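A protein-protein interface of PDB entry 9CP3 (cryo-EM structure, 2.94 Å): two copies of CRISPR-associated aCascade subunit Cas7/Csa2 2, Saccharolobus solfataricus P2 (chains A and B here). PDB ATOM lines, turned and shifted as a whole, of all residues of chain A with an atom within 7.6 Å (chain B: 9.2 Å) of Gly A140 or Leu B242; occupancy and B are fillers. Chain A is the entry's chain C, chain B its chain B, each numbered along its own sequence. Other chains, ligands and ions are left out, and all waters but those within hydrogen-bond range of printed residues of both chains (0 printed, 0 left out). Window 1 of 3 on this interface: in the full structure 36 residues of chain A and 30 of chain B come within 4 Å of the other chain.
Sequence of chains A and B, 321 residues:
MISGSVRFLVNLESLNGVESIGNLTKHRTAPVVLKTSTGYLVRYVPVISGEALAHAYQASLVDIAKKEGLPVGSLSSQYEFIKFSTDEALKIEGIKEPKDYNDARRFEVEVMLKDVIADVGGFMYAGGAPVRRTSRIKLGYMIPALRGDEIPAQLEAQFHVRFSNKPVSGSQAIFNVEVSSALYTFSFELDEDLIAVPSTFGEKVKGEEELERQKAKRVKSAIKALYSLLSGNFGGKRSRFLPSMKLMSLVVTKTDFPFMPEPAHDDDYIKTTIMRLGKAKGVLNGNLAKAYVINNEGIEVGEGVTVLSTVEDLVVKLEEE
The guanidinium group (NH1) of Arg B238 is in hydrogen-bond range of the side-chain sulfur (SD) of Met A260, 3.7 Å away.
The backbone carbonyl oxygen (O) of Ser B239 sits at hydrogen-bond distance from the backbone NH (N) of Leu A139 (2.8 Å).
The backbone NH of Leu B242 is in hydrogen-bond range of the backbone carbonyl oxygen of Leu A139 (3.1 Å).
The backbone carbonyl oxygen (O) of Leu A139 sits at hydrogen-bond distance from the backbone NH (N) of Phe B241, at 3.5 Å.
O of Leu A139 sits close to O of Arg B240 (3.4 Å).
ND2 of Asn B233 lies within hydrogen-bond range of SD of Met A260, 3.1 Å away.
O of Gly B235 is in hydrogen-bond range of NE of Arg B238.
O of Ile A143 lies within hydrogen-bond range of N of Thr A185 (3.0 Å).
The backbone carbonyl oxygen (O) of Glu A189 sits at hydrogen-bond distance from the backbone NH (N) of Lys A138, at 2.9 Å.
The guanidinium group (NH2) of Arg B238 lies within hydrogen-bond range of the backbone carbonyl oxygen (O) of Gly B232 (2.9 Å).
Lys A138 touches Arg B238 (CB to O, 3.6 Å).
Ser B239 touches Lys A138.
Arg B240 touches Gly A140.
Leu B242 touches Gly A140.
CE1 of Tyr A141 touches CD1 of Phe B241 (3.5 Å).
Leu B12 touches Ile A143.
CD2 of Leu B242 touches OG of Ser A187, at 3.4 Å.
Of chain B, only Arg B240 and Leu B242 come within 4 Å of Gly A140.
Of chain A, only Leu A139, Gly A140 and Ser A187 come within 4 Å of Leu B242.
Printed residues of chain B within 4 Å of Met A260: Asn B233 and Arg B238.
Of the printed residues of chain B, Leu A139 touches Ser B239 (2.8 Å), Arg B240 (3.1 Å), Phe B241 (3.5 Å) and Leu B242 (3.1 Å).
The nearest residue of chain A that does not touch Leu B242 is Lys A138 (4.6 Å).
Of the 20 printed residues of chain B, 7 touch a printed residue of chain A.
Printed residues of chain B that touch a printed residue of chain A: Leu B12, Asn B233, Arg B238, Ser B239, Arg B240, Phe B241 and Leu B242.
Hydrophobic or aromatic side chains of chain B within 4 Å of the printed part of chain A: Leu B12, Phe B241 and Leu B242.
Along chain B the printed residues that touch a printed residue of chain A span positions 12 to 242.
Among the printed residues, 13 pairs touch across the chains.
No position is printed for both chains.
Of the 13 pairs that touch across the chains among the printed residues, none has its exchanged pair printed and touching as well.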
ATOM      1  N   GLY A   4     -39.780  -6.292   8.026  1.00  0.00           N
ATOM      2  CA  GLY A   4     -40.261  -6.476   9.381  1.00  0.00           C
ATOM      3  C   GLY A   4     -39.244  -6.068  10.419  1.00  0.00           C
ATOM      4  O   GLY A   4     -38.046  -5.963  10.141  1.00  0.00           O
ATOM      5  N   ILE A  48     -24.646  -9.246  18.605  1.00  0.00           N
ATOM      6  CA  ILE A  48     -24.607 -10.501  17.864  1.00  0.00           C
ATOM      7  C   ILE A  48     -24.590 -10.173  16.377  1.00  0.00           C
ATOM      8  O   ILE A  48     -25.421  -9.392  15.900  1.00  0.00           O
ATOM      9  CB  ILE A  48     -25.806 -11.406  18.206  1.00  0.00           C
ATOM     10  CG1 ILE A  48     -25.668 -11.970  19.620  1.00  0.00           C
ATOM     11  CG2 ILE A  48     -25.931 -12.531  17.198  1.00  0.00           C
ATOM     12  CD1 ILE A  48     -26.979 -12.405  20.230  1.00  0.00           C
ATOM     13  N   SER A  49     -23.651 -10.770  15.652  1.00  0.00           N
ATOM     14  CA  SER A  49     -23.490 -10.490  14.235  1.00  0.00           C
ATOM     15  C   SER A  49     -24.610 -11.131  13.421  1.00  0.00           C
ATOM     16  O   SER A  49     -25.301 -12.045  13.873  1.00  0.00           O
ATOM     17  CB  SER A  49     -22.135 -10.986  13.737  1.00  0.00           C
ATOM     18  OG  SER A  49     -22.113 -12.398  13.651  1.00  0.00           O
ATOM     19  N   GLY A  50     -24.786 -10.626  12.200  1.00  0.00           N
ATOM     20  CA  GLY A  50     -25.793 -11.144  11.297  1.00  0.00           C
ATOM     21  C   GLY A  50     -25.360 -12.336  10.480  1.00  0.00           C
ATOM     22  O   GLY A  50     -26.187 -12.938   9.789  1.00  0.00           O
ATOM     23  N   GLU A  51     -24.074 -12.687  10.536  1.00  0.00           N
ATOM     24  CA  GLU A  51     -23.575 -13.842   9.796  1.00  0.00           C
ATOM     25  C   GLU A  51     -24.208 -15.136  10.295  1.00  0.00           C
ATOM     26  O   GLU A  51     -24.553 -16.016   9.498  1.00  0.00           O
ATOM     27  CB  GLU A  51     -22.054 -13.912   9.906  1.00  0.00           C
ATOM     28  CG  GLU A  51     -21.333 -12.678   9.394  1.00  0.00           C
ATOM     29  CD  GLU A  51     -21.148 -12.684   7.891  1.00  0.00           C
ATOM     30  OE1 GLU A  51     -21.718 -13.567   7.219  1.00  0.00           O
ATOM     31  OE2 GLU A  51     -20.426 -11.803   7.379  1.00  0.00           O
ATOM     32  N   LEU A  53     -27.182 -15.426  11.669  1.00  0.00           N
ATOM     33  CA  LEU A  53     -28.561 -15.445  11.193  1.00  0.00           C
ATOM     34  C   LEU A  53     -28.637 -15.930   9.750  1.00  0.00           C
ATOM     35  O   LEU A  53     -29.486 -16.762   9.405  1.00  0.00           O
ATOM     36  CB  LEU A  53     -29.174 -14.052  11.325  1.00  0.00           C
ATOM     37  CG  LEU A  53     -28.978 -13.347  12.668  1.00  0.00           C
ATOM     38  CD1 LEU A  53     -29.457 -11.910  12.581  1.00  0.00           C
ATOM     39  CD2 LEU A  53     -29.701 -14.085  13.774  1.00  0.00           C
ATOM     40  N   LYS A 138     -31.892  -9.626   3.659  1.00  0.00           N
ATOM     41  CA  LYS A 138     -30.990  -8.664   4.274  1.00  0.00           C
ATOM     42  C   LYS A 138     -31.199  -8.670   5.781  1.00  0.00           C
ATOM     43  O   LYS A 138     -32.338  -8.612   6.255  1.00  0.00           O
ATOM     44  CB  LYS A 138     -31.210  -7.263   3.703  1.00  0.00           C
ATOM     45  CG  LYS A 138     -31.240  -7.232   2.189  1.00  0.00           C
ATOM     46  CD  LYS A 138     -31.207  -5.814   1.661  1.00  0.00           C
ATOM     47  CE  LYS A 138     -31.067  -5.802   0.148  1.00  0.00           C
ATOM     48  NZ  LYS A 138     -29.688  -6.165  -0.278  1.00  0.00           N
ATOM     49  N   LEU A 139     -30.098  -8.741   6.525  1.00  0.00           N
ATOM     50  CA  LEU A 139     -30.121  -8.786   7.977  1.00  0.00           C
ATOM     51  C   LEU A 139     -29.095  -7.809   8.531  1.00  0.00           C
ATOM     52  O   LEU A 139     -28.319  -7.197   7.791  1.00  0.00           O
ATOM     53  CB  LEU A 139     -29.847 -10.205   8.489  1.00  0.00           C
ATOM     54  CG  LEU A 139     -30.980 -11.205   8.259  1.00  0.00           C
ATOM     55  CD1 LEU A 139     -30.446 -12.622   8.237  1.00  0.00           C
ATOM     56  CD2 LEU A 139     -32.038 -11.053   9.338  1.00  0.00           C
ATOM     57  N   GLY A 140     -29.092  -7.668   9.855  1.00  0.00           N
ATOM     58  CA  GLY A 140     -28.175  -6.769  10.520  1.00  0.00           C
ATOM     59  C   GLY A 140     -27.810  -7.283  11.896  1.00  0.00           C
ATOM     60  O   GLY A 140     -28.308  -8.314  12.350  1.00  0.00           O
ATOM     61  N   TYR A 141     -26.922  -6.545  12.559  1.00  0.00           N
ATOM     62  CA  TYR A 141     -26.499  -6.904  13.905  1.00  0.00           C
ATOM     63  C   TYR A 141     -27.675  -6.856  14.871  1.00  0.00           C
ATOM     64  O   TYR A 141     -28.565  -6.012  14.753  1.00  0.00           O
ATOM     65  CB  TYR A 141     -25.403  -5.956  14.387  1.00  0.00           C
ATOM     66  CG  TYR A 141     -23.998  -6.378  14.043  1.00  0.00           C
ATOM     67  CD1 TYR A 141     -23.565  -6.413  12.726  1.00  0.00           C
ATOM     68  CD2 TYR A 141     -23.095  -6.722  15.037  1.00  0.00           C
ATOM     69  CE1 TYR A 141     -22.275  -6.791  12.411  1.00  0.00           C
ATOM     70  CE2 TYR A 141     -21.807  -7.100  14.732  1.00  0.00           C
ATOM     71  CZ  TYR A 141     -21.401  -7.133  13.419  1.00  0.00           C
ATOM     72  OH  TYR A 141     -20.116  -7.511  13.113  1.00  0.00           O
ATOM     73  N   MET A 142     -27.676  -7.776  15.830  1.00  0.00           N
ATOM     74  CA  MET A 142     -28.705  -7.820  16.862  1.00  0.00           C
ATOM     75  C   MET A 142     -28.226  -6.973  18.038  1.00  0.00           C
ATOM     76  O   MET A 142     -27.252  -7.326  18.710  1.00  0.00           O
ATOM     77  CB  MET A 142     -28.983  -9.262  17.276  1.00  0.00           C
ATOM     78  CG  MET A 142     -30.416  -9.516  17.689  1.00  0.00           C
ATOM     79  SD  MET A 142     -30.672 -11.176  18.331  1.00  0.00           S
ATOM     80  CE  MET A 142     -30.857 -12.087  16.802  1.00  0.00           C
ATOM     81  N   ILE A 143     -28.913  -5.863  18.289  1.00  0.00           N
ATOM     82  CA  ILE A 143     -28.436  -4.843  19.221  1.00  0.00           C
ATOM     83  C   ILE A 143     -29.413  -4.694  20.381  1.00  0.00           C
ATOM     84  O   ILE A 143     -30.632  -4.721  20.162  1.00  0.00           O
ATOM     85  CB  ILE A 143     -28.239  -3.498  18.505  1.00  0.00           C
ATOM     86  CG1 ILE A 143     -27.426  -3.696  17.229  1.00  0.00           C
ATOM     87  CG2 ILE A 143     -27.560  -2.493  19.414  1.00  0.00           C
ATOM     88  CD1 ILE A 143     -26.091  -4.330  17.481  1.00  0.00           C
ATOM     89  N   THR A 185     -33.042  -6.417  19.579  1.00  0.00           N
ATOM     90  CA  THR A 185     -33.993  -5.988  18.566  1.00  0.00           C
ATOM     91  C   THR A 185     -33.331  -6.088  17.202  1.00  0.00           C
ATOM     92  O   THR A 185     -32.146  -5.771  17.069  1.00  0.00           O
ATOM     93  CB  THR A 185     -34.454  -4.539  18.785  1.00  0.00           C
ATOM     94  OG1 THR A 185     -33.355  -3.651  18.552  1.00  0.00           O
ATOM     95  CG2 THR A 185     -34.959  -4.331  20.202  1.00  0.00           C
ATOM     96  N   PHE A 186     -34.082  -6.519  16.190  1.00  0.00           N
ATOM     97  CA  PHE A 186     -33.515  -6.510  14.846  1.00  0.00           C
ATOM     98  C   PHE A 186     -34.622  -6.504  13.801  1.00  0.00           C
ATOM     99  O   PHE A 186     -35.781  -6.814  14.086  1.00  0.00           O
ATOM    100  CB  PHE A 186     -32.557  -7.691  14.623  1.00  0.00           C
ATOM    101  CG  PHE A 186     -33.239  -9.002  14.348  1.00  0.00           C
ATOM    102  CD1 PHE A 186     -33.762  -9.755  15.385  1.00  0.00           C
ATOM    103  CD2 PHE A 186     -33.334  -9.494  13.056  1.00  0.00           C
ATOM    104  CE1 PHE A 186     -34.374 -10.967  15.139  1.00  0.00           C
ATOM    105  CE2 PHE A 186     -33.951 -10.702  12.802  1.00  0.00           C
ATOM    106  CZ  PHE A 186     -34.473 -11.439  13.845  1.00  0.00           C
ATOM    107  N   SER A 187     -34.235  -6.144  12.579  1.00  0.00           N
ATOM    108  CA  SER A 187     -35.152  -6.002  11.460  1.00  0.00           C
ATOM    109  C   SER A 187     -34.610  -6.759  10.254  1.00  0.00           C
ATOM    110  O   SER A 187     -33.409  -7.010  10.140  1.00  0.00           O
ATOM    111  CB  SER A 187     -35.376  -4.526  11.106  1.00  0.00           C
ATOM    112  OG  SER A 187     -34.157  -3.898  10.749  1.00  0.00           O
ATOM    113  N   PHE A 188     -35.516  -7.113   9.345  1.00  0.00           N
ATOM    114  CA  PHE A 188     -35.165  -7.904   8.174  1.00  0.00           C
ATOM    115  C   PHE A 188     -35.988  -7.463   6.972  1.00  0.00           C
ATOM    116  O   PHE A 188     -37.043  -6.834   7.105  1.00  0.00           O
ATOM    117  CB  PHE A 188     -35.372  -9.404   8.422  1.00  0.00           C
ATOM    118  CG  PHE A 188     -36.814  -9.820   8.463  1.00  0.00           C
ATOM    119  CD1 PHE A 188     -37.536  -9.732   9.638  1.00  0.00           C
ATOM    120  CD2 PHE A 188     -37.444 -10.306   7.330  1.00  0.00           C
ATOM    121  CE1 PHE A 188     -38.860 -10.114   9.684  1.00  0.00           C
ATOM    122  CE2 PHE A 188     -38.768 -10.689   7.369  1.00  0.00           C
ATOM    123  CZ  PHE A 188     -39.478 -10.593   8.547  1.00  0.00           C
ATOM    124  N   GLU A 189     -35.481  -7.812   5.789  1.00  0.00           N
ATOM    125  CA  GLU A 189     -36.108  -7.489   4.516  1.00  0.00           C
ATOM    126  C   GLU A 189     -35.887  -8.638   3.541  1.00  0.00           C
ATOM    127  O   GLU A 189     -34.793  -9.204   3.480  1.00  0.00           O
ATOM    128  CB  GLU A 189     -35.541  -6.187   3.936  1.00  0.00           C
ATOM    129  CG  GLU A 189     -35.652  -6.067   2.426  1.00  0.00           C
ATOM    130  CD  GLU A 189     -35.116  -4.748   1.908  1.00  0.00           C
ATOM    131  OE1 GLU A 189     -34.808  -3.864   2.734  1.00  0.00           O
ATOM    132  OE2 GLU A 189     -34.995  -4.599   0.674  1.00  0.00           O
ATOM    133  N   MET A 260     -39.004   0.913   4.586  1.00  0.00           N
ATOM    134  CA  MET A 260     -38.224   0.450   5.728  1.00  0.00           C
ATOM    135  C   MET A 260     -38.968   0.756   7.021  1.00  0.00           C
ATOM    136  O   MET A 260     -39.236   1.935   7.310  1.00  0.00           O
ATOM    137  CB  MET A 260     -36.841   1.103   5.742  1.00  0.00           C
ATOM    138  CG  MET A 260     -35.757   0.277   5.075  1.00  0.00           C
ATOM    139  SD  MET A 260     -34.260   1.231   4.770  1.00  0.00           S
ATOM    140  CE  MET A 260     -34.120   2.139   6.307  1.00  0.00           C
ATOM    141  N   PRO A 261     -39.313  -0.246   7.822  1.00  0.00           N
ATOM    142  CA  PRO A 261     -40.028   0.018   9.074  1.00  0.00           C
ATOM    143  C   PRO A 261     -39.122   0.666  10.109  1.00  0.00           C
ATOM    144  O   PRO A 261     -37.892   0.623  10.020  1.00  0.00           O
ATOM    145  CB  PRO A 261     -40.481  -1.372   9.523  1.00  0.00           C
ATOM    146  CG  PRO A 261     -39.484  -2.293   8.921  1.00  0.00           C
ATOM    147  CD  PRO A 261     -39.079  -1.682   7.609  1.00  0.00           C
ATOM    148  N   VAL B  10     -26.822   6.863  13.710  1.00  0.00           N
ATOM    149  CA  VAL B  10     -26.512   5.595  13.062  1.00  0.00           C
ATOM    150  C   VAL B  10     -25.654   4.762  14.001  1.00  0.00           C
ATOM    151  O   VAL B  10     -24.683   5.266  14.576  1.00  0.00           O
ATOM    152  CB  VAL B  10     -25.800   5.809  11.714  1.00  0.00           C
ATOM    153  CG1 VAL B  10     -25.784   4.522  10.921  1.00  0.00           C
ATOM    154  CG2 VAL B  10     -26.479   6.911  10.924  1.00  0.00           C
ATOM    155  N   ASN B  11     -26.030   3.497  14.175  1.00  0.00           N
ATOM    156  CA  ASN B  11     -25.340   2.594  15.084  1.00  0.00           C
ATOM    157  C   ASN B  11     -25.062   1.276  14.377  1.00  0.00           C
ATOM    158  O   ASN B  11     -25.927   0.744  13.676  1.00  0.00           O
ATOM    159  CB  ASN B  11     -26.168   2.344  16.345  1.00  0.00           C
ATOM    160  CG  ASN B  11     -26.202   3.544  17.262  1.00  0.00           C
ATOM    161  OD1 ASN B  11     -25.162   4.063  17.661  1.00  0.00           O
ATOM    162  ND2 ASN B  11     -27.402   3.993  17.603  1.00  0.00           N
ATOM    163  N   LEU B  12     -23.851   0.754  14.579  1.00  0.00           N
ATOM    164  CA  LEU B  12     -23.426  -0.530  14.021  1.00  0.00           C
ATOM    165  C   LEU B  12     -23.556  -0.531  12.497  1.00  0.00           C
ATOM    166  O   LEU B  12     -24.322  -1.293  11.906  1.00  0.00           O
ATOM    167  CB  LEU B  12     -24.210  -1.691  14.643  1.00  0.00           C
ATOM    168  CG  LEU B  12     -23.711  -2.258  15.974  1.00  0.00           C
ATOM    169  CD1 LEU B  12     -22.328  -2.868  15.823  1.00  0.00           C
ATOM    170  CD2 LEU B  12     -23.740  -1.225  17.095  1.00  0.00           C
ATOM    171  N   GLU B  13     -22.781   0.344  11.865  1.00  0.00           N
ATOM    172  CA  GLU B  13     -22.881   0.576  10.434  1.00  0.00           C
ATOM    173  C   GLU B  13     -21.529   0.391   9.763  1.00  0.00           C
ATOM    174  O   GLU B  13     -20.481   0.696  10.337  1.00  0.00           O
ATOM    175  CB  GLU B  13     -23.418   1.980  10.133  1.00  0.00           C
ATOM    176  CG  GLU B  13     -22.496   3.115  10.558  1.00  0.00           C
ATOM    177  CD  GLU B  13     -21.571   3.569   9.446  1.00  0.00           C
ATOM    178  OE1 GLU B  13     -21.888   3.314   8.267  1.00  0.00           O
ATOM    179  OE2 GLU B  13     -20.524   4.179   9.752  1.00  0.00           O
ATOM    180  N   SER B  14     -21.571  -0.126   8.537  1.00  0.00           N
ATOM    181  CA  SER B  14     -20.425  -0.127   7.625  1.00  0.00           C
ATOM    182  C   SER B  14     -20.995   0.219   6.252  1.00  0.00           C
ATOM    183  O   SER B  14     -21.369  -0.669   5.482  1.00  0.00           O
ATOM    184  CB  SER B  14     -19.699  -1.464   7.623  1.00  0.00           C
ATOM    185  OG  SER B  14     -18.542  -1.405   6.811  1.00  0.00           O
ATOM    186  N   LEU B  15     -21.056   1.517   5.952  1.00  0.00           N
ATOM    187  CA  LEU B  15     -21.726   2.005   4.757  1.00  0.00           C
ATOM    188  C   LEU B  15     -20.778   2.498   3.676  1.00  0.00           C
ATOM    189  O   LEU B  15     -21.181   2.563   2.511  1.00  0.00           O
ATOM    190  CB  LEU B  15     -22.698   3.135   5.120  1.00  0.00           C
ATOM    191  CG  LEU B  15     -24.147   2.713   5.370  1.00  0.00           C
ATOM    192  CD1 LEU B  15     -24.266   1.838   6.603  1.00  0.00           C
ATOM    193  CD2 LEU B  15     -25.021   3.937   5.514  1.00  0.00           C
ATOM    194  N   VAL B 179     -16.448  -1.375  12.023  1.00  0.00           N
ATOM    195  CA  VAL B 179     -17.817  -0.971  12.317  1.00  0.00           C
ATOM    196  C   VAL B 179     -17.783   0.307  13.146  1.00  0.00           C
ATOM    197  O   VAL B 179     -16.991   0.428  14.089  1.00  0.00           O
ATOM    198  CB  VAL B 179     -18.590  -2.083  13.057  1.00  0.00           C
ATOM    199  CG1 VAL B 179     -19.970  -1.600  13.449  1.00  0.00           C
ATOM    200  CG2 VAL B 179     -18.689  -3.328  12.191  1.00  0.00           C
ATOM    201  N   GLY B 232     -33.215   7.028   4.030  1.00  0.00           N
ATOM    202  CA  GLY B 232     -31.986   6.380   4.440  1.00  0.00           C
ATOM    203  C   GLY B 232     -31.660   5.076   3.742  1.00  0.00           C
ATOM    204  O   GLY B 232     -31.192   4.132   4.386  1.00  0.00           O
ATOM    205  N   ASN B 233     -31.896   4.998   2.434  1.00  0.00           N
ATOM    206  CA  ASN B 233     -31.472   3.851   1.634  1.00  0.00           C
ATOM    207  C   ASN B 233     -30.402   4.334   0.660  1.00  0.00           C
ATOM    208  O   ASN B 233     -30.672   4.605  -0.511  1.00  0.00           O
ATOM    209  CB  ASN B 233     -32.656   3.226   0.895  1.00  0.00           C
ATOM    210  CG  ASN B 233     -33.794   2.860   1.820  1.00  0.00           C
ATOM    211  OD1 ASN B 233     -34.260   3.684   2.604  1.00  0.00           O
ATOM    212  ND2 ASN B 233     -34.250   1.617   1.734  1.00  0.00           N
ATOM    213  N   GLY B 235     -26.538   3.481   1.666  1.00  0.00           N
ATOM    214  CA  GLY B 235     -25.248   2.875   1.919  1.00  0.00           C
ATOM    215  C   GLY B 235     -25.136   1.455   1.393  1.00  0.00           C
ATOM    216  O   GLY B 235     -26.126   0.778   1.124  1.00  0.00           O
ATOM    217  N   GLY B 236     -23.889   1.000   1.255  1.00  0.00           N
ATOM    218  CA  GLY B 236     -23.605  -0.360   0.850  1.00  0.00           C
ATOM    219  C   GLY B 236     -23.444  -1.301   2.029  1.00  0.00           C
ATOM    220  O   GLY B 236     -23.664  -0.944   3.188  1.00  0.00           O
ATOM    221  N   LYS B 237     -23.039  -2.533   1.710  1.00  0.00           N
ATOM    222  CA  LYS B 237     -22.908  -3.606   2.700  1.00  0.00           C
ATOM    223  C   LYS B 237     -24.204  -3.770   3.487  1.00  0.00           C
ATOM    224  O   LYS B 237     -24.203  -3.972   4.703  1.00  0.00           O
ATOM    225  CB  LYS B 237     -21.722  -3.373   3.636  1.00  0.00           C
ATOM    226  CG  LYS B 237     -20.417  -3.947   3.119  1.00  0.00           C
ATOM    227  CD  LYS B 237     -19.366  -4.008   4.209  1.00  0.00           C
ATOM    228  CE  LYS B 237     -17.971  -4.064   3.614  1.00  0.00           C
ATOM    229  NZ  LYS B 237     -17.876  -5.100   2.551  1.00  0.00           N
ATOM    230  N   ARG B 238     -25.322  -3.678   2.776  1.00  0.00           N
ATOM    231  CA  ARG B 238     -26.644  -3.695   3.382  1.00  0.00           C
ATOM    232  C   ARG B 238     -27.208  -5.101   3.544  1.00  0.00           C
ATOM    233  O   ARG B 238     -28.250  -5.265   4.185  1.00  0.00           O
ATOM    234  CB  ARG B 238     -27.596  -2.837   2.541  1.00  0.00           C
ATOM    235  CG  ARG B 238     -28.796  -2.289   3.288  1.00  0.00           C
ATOM    236  CD  ARG B 238     -29.534  -1.275   2.429  1.00  0.00           C
ATOM    237  NE  ARG B 238     -29.135   0.092   2.741  1.00  0.00           N
ATOM    238  CZ  ARG B 238     -29.694   0.840   3.681  1.00  0.00           C
ATOM    239  NH1 ARG B 238     -30.688   0.387   4.426  1.00  0.00           N
ATOM    240  NH2 ARG B 238     -29.241   2.075   3.882  1.00  0.00           N
ATOM    241  N   SER B 239     -26.544  -6.117   2.987  1.00  0.00           N
ATOM    242  CA  SER B 239     -27.074  -7.475   3.052  1.00  0.00           C
ATOM    243  C   SER B 239     -26.916  -8.073   4.445  1.00  0.00           C
ATOM    244  O   SER B 239     -27.821  -8.754   4.938  1.00  0.00           O
ATOM    245  CB  SER B 239     -26.389  -8.356   2.009  1.00  0.00           C
ATOM    246  OG  SER B 239     -25.026  -8.564   2.332  1.00  0.00           O
ATOM    247  N   ARG B 240     -25.779  -7.832   5.096  1.00  0.00           N
ATOM    248  CA  ARG B 240     -25.509  -8.397   6.410  1.00  0.00           C
ATOM    249  C   ARG B 240     -25.203  -7.356   7.475  1.00  0.00           C
ATOM    250  O   ARG B 240     -25.066  -7.724   8.647  1.00  0.00           O
ATOM    251  CB  ARG B 240     -24.330  -9.382   6.336  1.00  0.00           C
ATOM    252  CG  ARG B 240     -24.460 -10.461   5.270  1.00  0.00           C
ATOM    253  CD  ARG B 240     -25.361 -11.595   5.732  1.00  0.00           C
ATOM    254  NE  ARG B 240     -25.570 -12.591   4.689  1.00  0.00           N
ATOM    255  CZ  ARG B 240     -26.623 -12.624   3.884  1.00  0.00           C
ATOM    256  NH1 ARG B 240     -27.592 -11.731   3.977  1.00  0.00           N
ATOM    257  NH2 ARG B 240     -26.706 -13.579   2.963  1.00  0.00           N
ATOM    258  N   PHE B 241     -25.100  -6.081   7.113  1.00  0.00           N
ATOM    259  CA  PHE B 241     -24.814  -4.992   8.041  1.00  0.00           C
ATOM    260  C   PHE B 241     -25.867  -3.900   7.913  1.00  0.00           C
ATOM    261  O   PHE B 241     -25.558  -2.715   7.780  1.00  0.00           O
ATOM    262  CB  PHE B 241     -23.417  -4.423   7.818  1.00  0.00           C
ATOM    263  CG  PHE B 241     -22.328  -5.455   7.860  1.00  0.00           C
ATOM    264  CD1 PHE B 241     -21.752  -5.821   9.064  1.00  0.00           C
ATOM    265  CD2 PHE B 241     -21.875  -6.055   6.698  1.00  0.00           C
ATOM    266  CE1 PHE B 241     -20.750  -6.768   9.110  1.00  0.00           C
ATOM    267  CE2 PHE B 241     -20.873  -7.003   6.737  1.00  0.00           C
ATOM    268  CZ  PHE B 241     -20.309  -7.360   7.944  1.00  0.00           C
ATOM    269  N   LEU B 242     -27.140  -4.301   7.929  1.00  0.00           N
ATOM    270  CA  LEU B 242     -28.264  -3.375   7.851  1.00  0.00           C
ATOM    271  C   LEU B 242     -28.185  -2.352   8.978  1.00  0.00           C
ATOM    272  O   LEU B 242     -28.376  -2.700  10.151  1.00  0.00           O
ATOM    273  CB  LEU B 242     -29.588  -4.139   7.915  1.00  0.00           C
ATOM    274  CG  LEU B 242     -30.854  -3.387   7.504  1.00  0.00           C
ATOM    275  CD1 LEU B 242     -30.964  -3.314   5.996  1.00  0.00           C
ATOM    276  CD2 LEU B 242     -32.086  -4.051   8.097  1.00  0.00           C
ATOM    277  N   PRO B 243     -27.909  -1.089   8.665  1.00  0.00           N
ATOM    278  CA  PRO B 243     -27.774  -0.081   9.721  1.00  0.00           C
ATOM    279  C   PRO B 243     -29.101   0.234  10.389  1.00  0.00           C
ATOM    280  O   PRO B 243     -30.175   0.095   9.799  1.00  0.00           O
ATOM    281  CB  PRO B 243     -27.228   1.138   8.974  1.00  0.00           C
ATOM    282  CG  PRO B 243     -27.740   0.974   7.588  1.00  0.00           C
ATOM    283  CD  PRO B 243     -27.765  -0.506   7.321  1.00  0.00           C
ATOM    284  N   SER B 244     -29.012   0.664  11.646  1.00  0.00           N
ATOM    285  CA  SER B 244     -30.164   1.118  12.414  1.00  0.00           C
ATOM    286  C   SER B 244     -30.168   2.642  12.387  1.00  0.00           C
ATOM    287  O   SER B 244     -29.317   3.281  13.014  1.00  0.00           O
ATOM    288  CB  SER B 244     -30.113   0.590  13.845  1.00  0.00           C
ATOM    289  OG  SER B 244     -31.016   1.295  14.675  1.00  0.00           O
ATOM    290  N   MET B 245     -31.120   3.223  11.664  1.00  0.00           N
ATOM    291  CA  MET B 245     -31.162   4.658  11.436  1.00  0.00           C
ATOM    292  C   MET B 245     -32.461   5.249  11.959  1.00  0.00           C
ATOM    293  O   MET B 245     -33.515   4.607  11.926  1.00  0.00           O
ATOM    294  CB  MET B 245     -31.015   4.982   9.947  1.00  0.00           C
ATOM    295  CG  MET B 245     -29.602   4.826   9.428  1.00  0.00           C
ATOM    296  SD  MET B 245     -29.346   5.619   7.835  1.00  0.00           S
ATOM    297  CE  MET B 245     -27.575   5.428   7.663  1.00  0.00           C
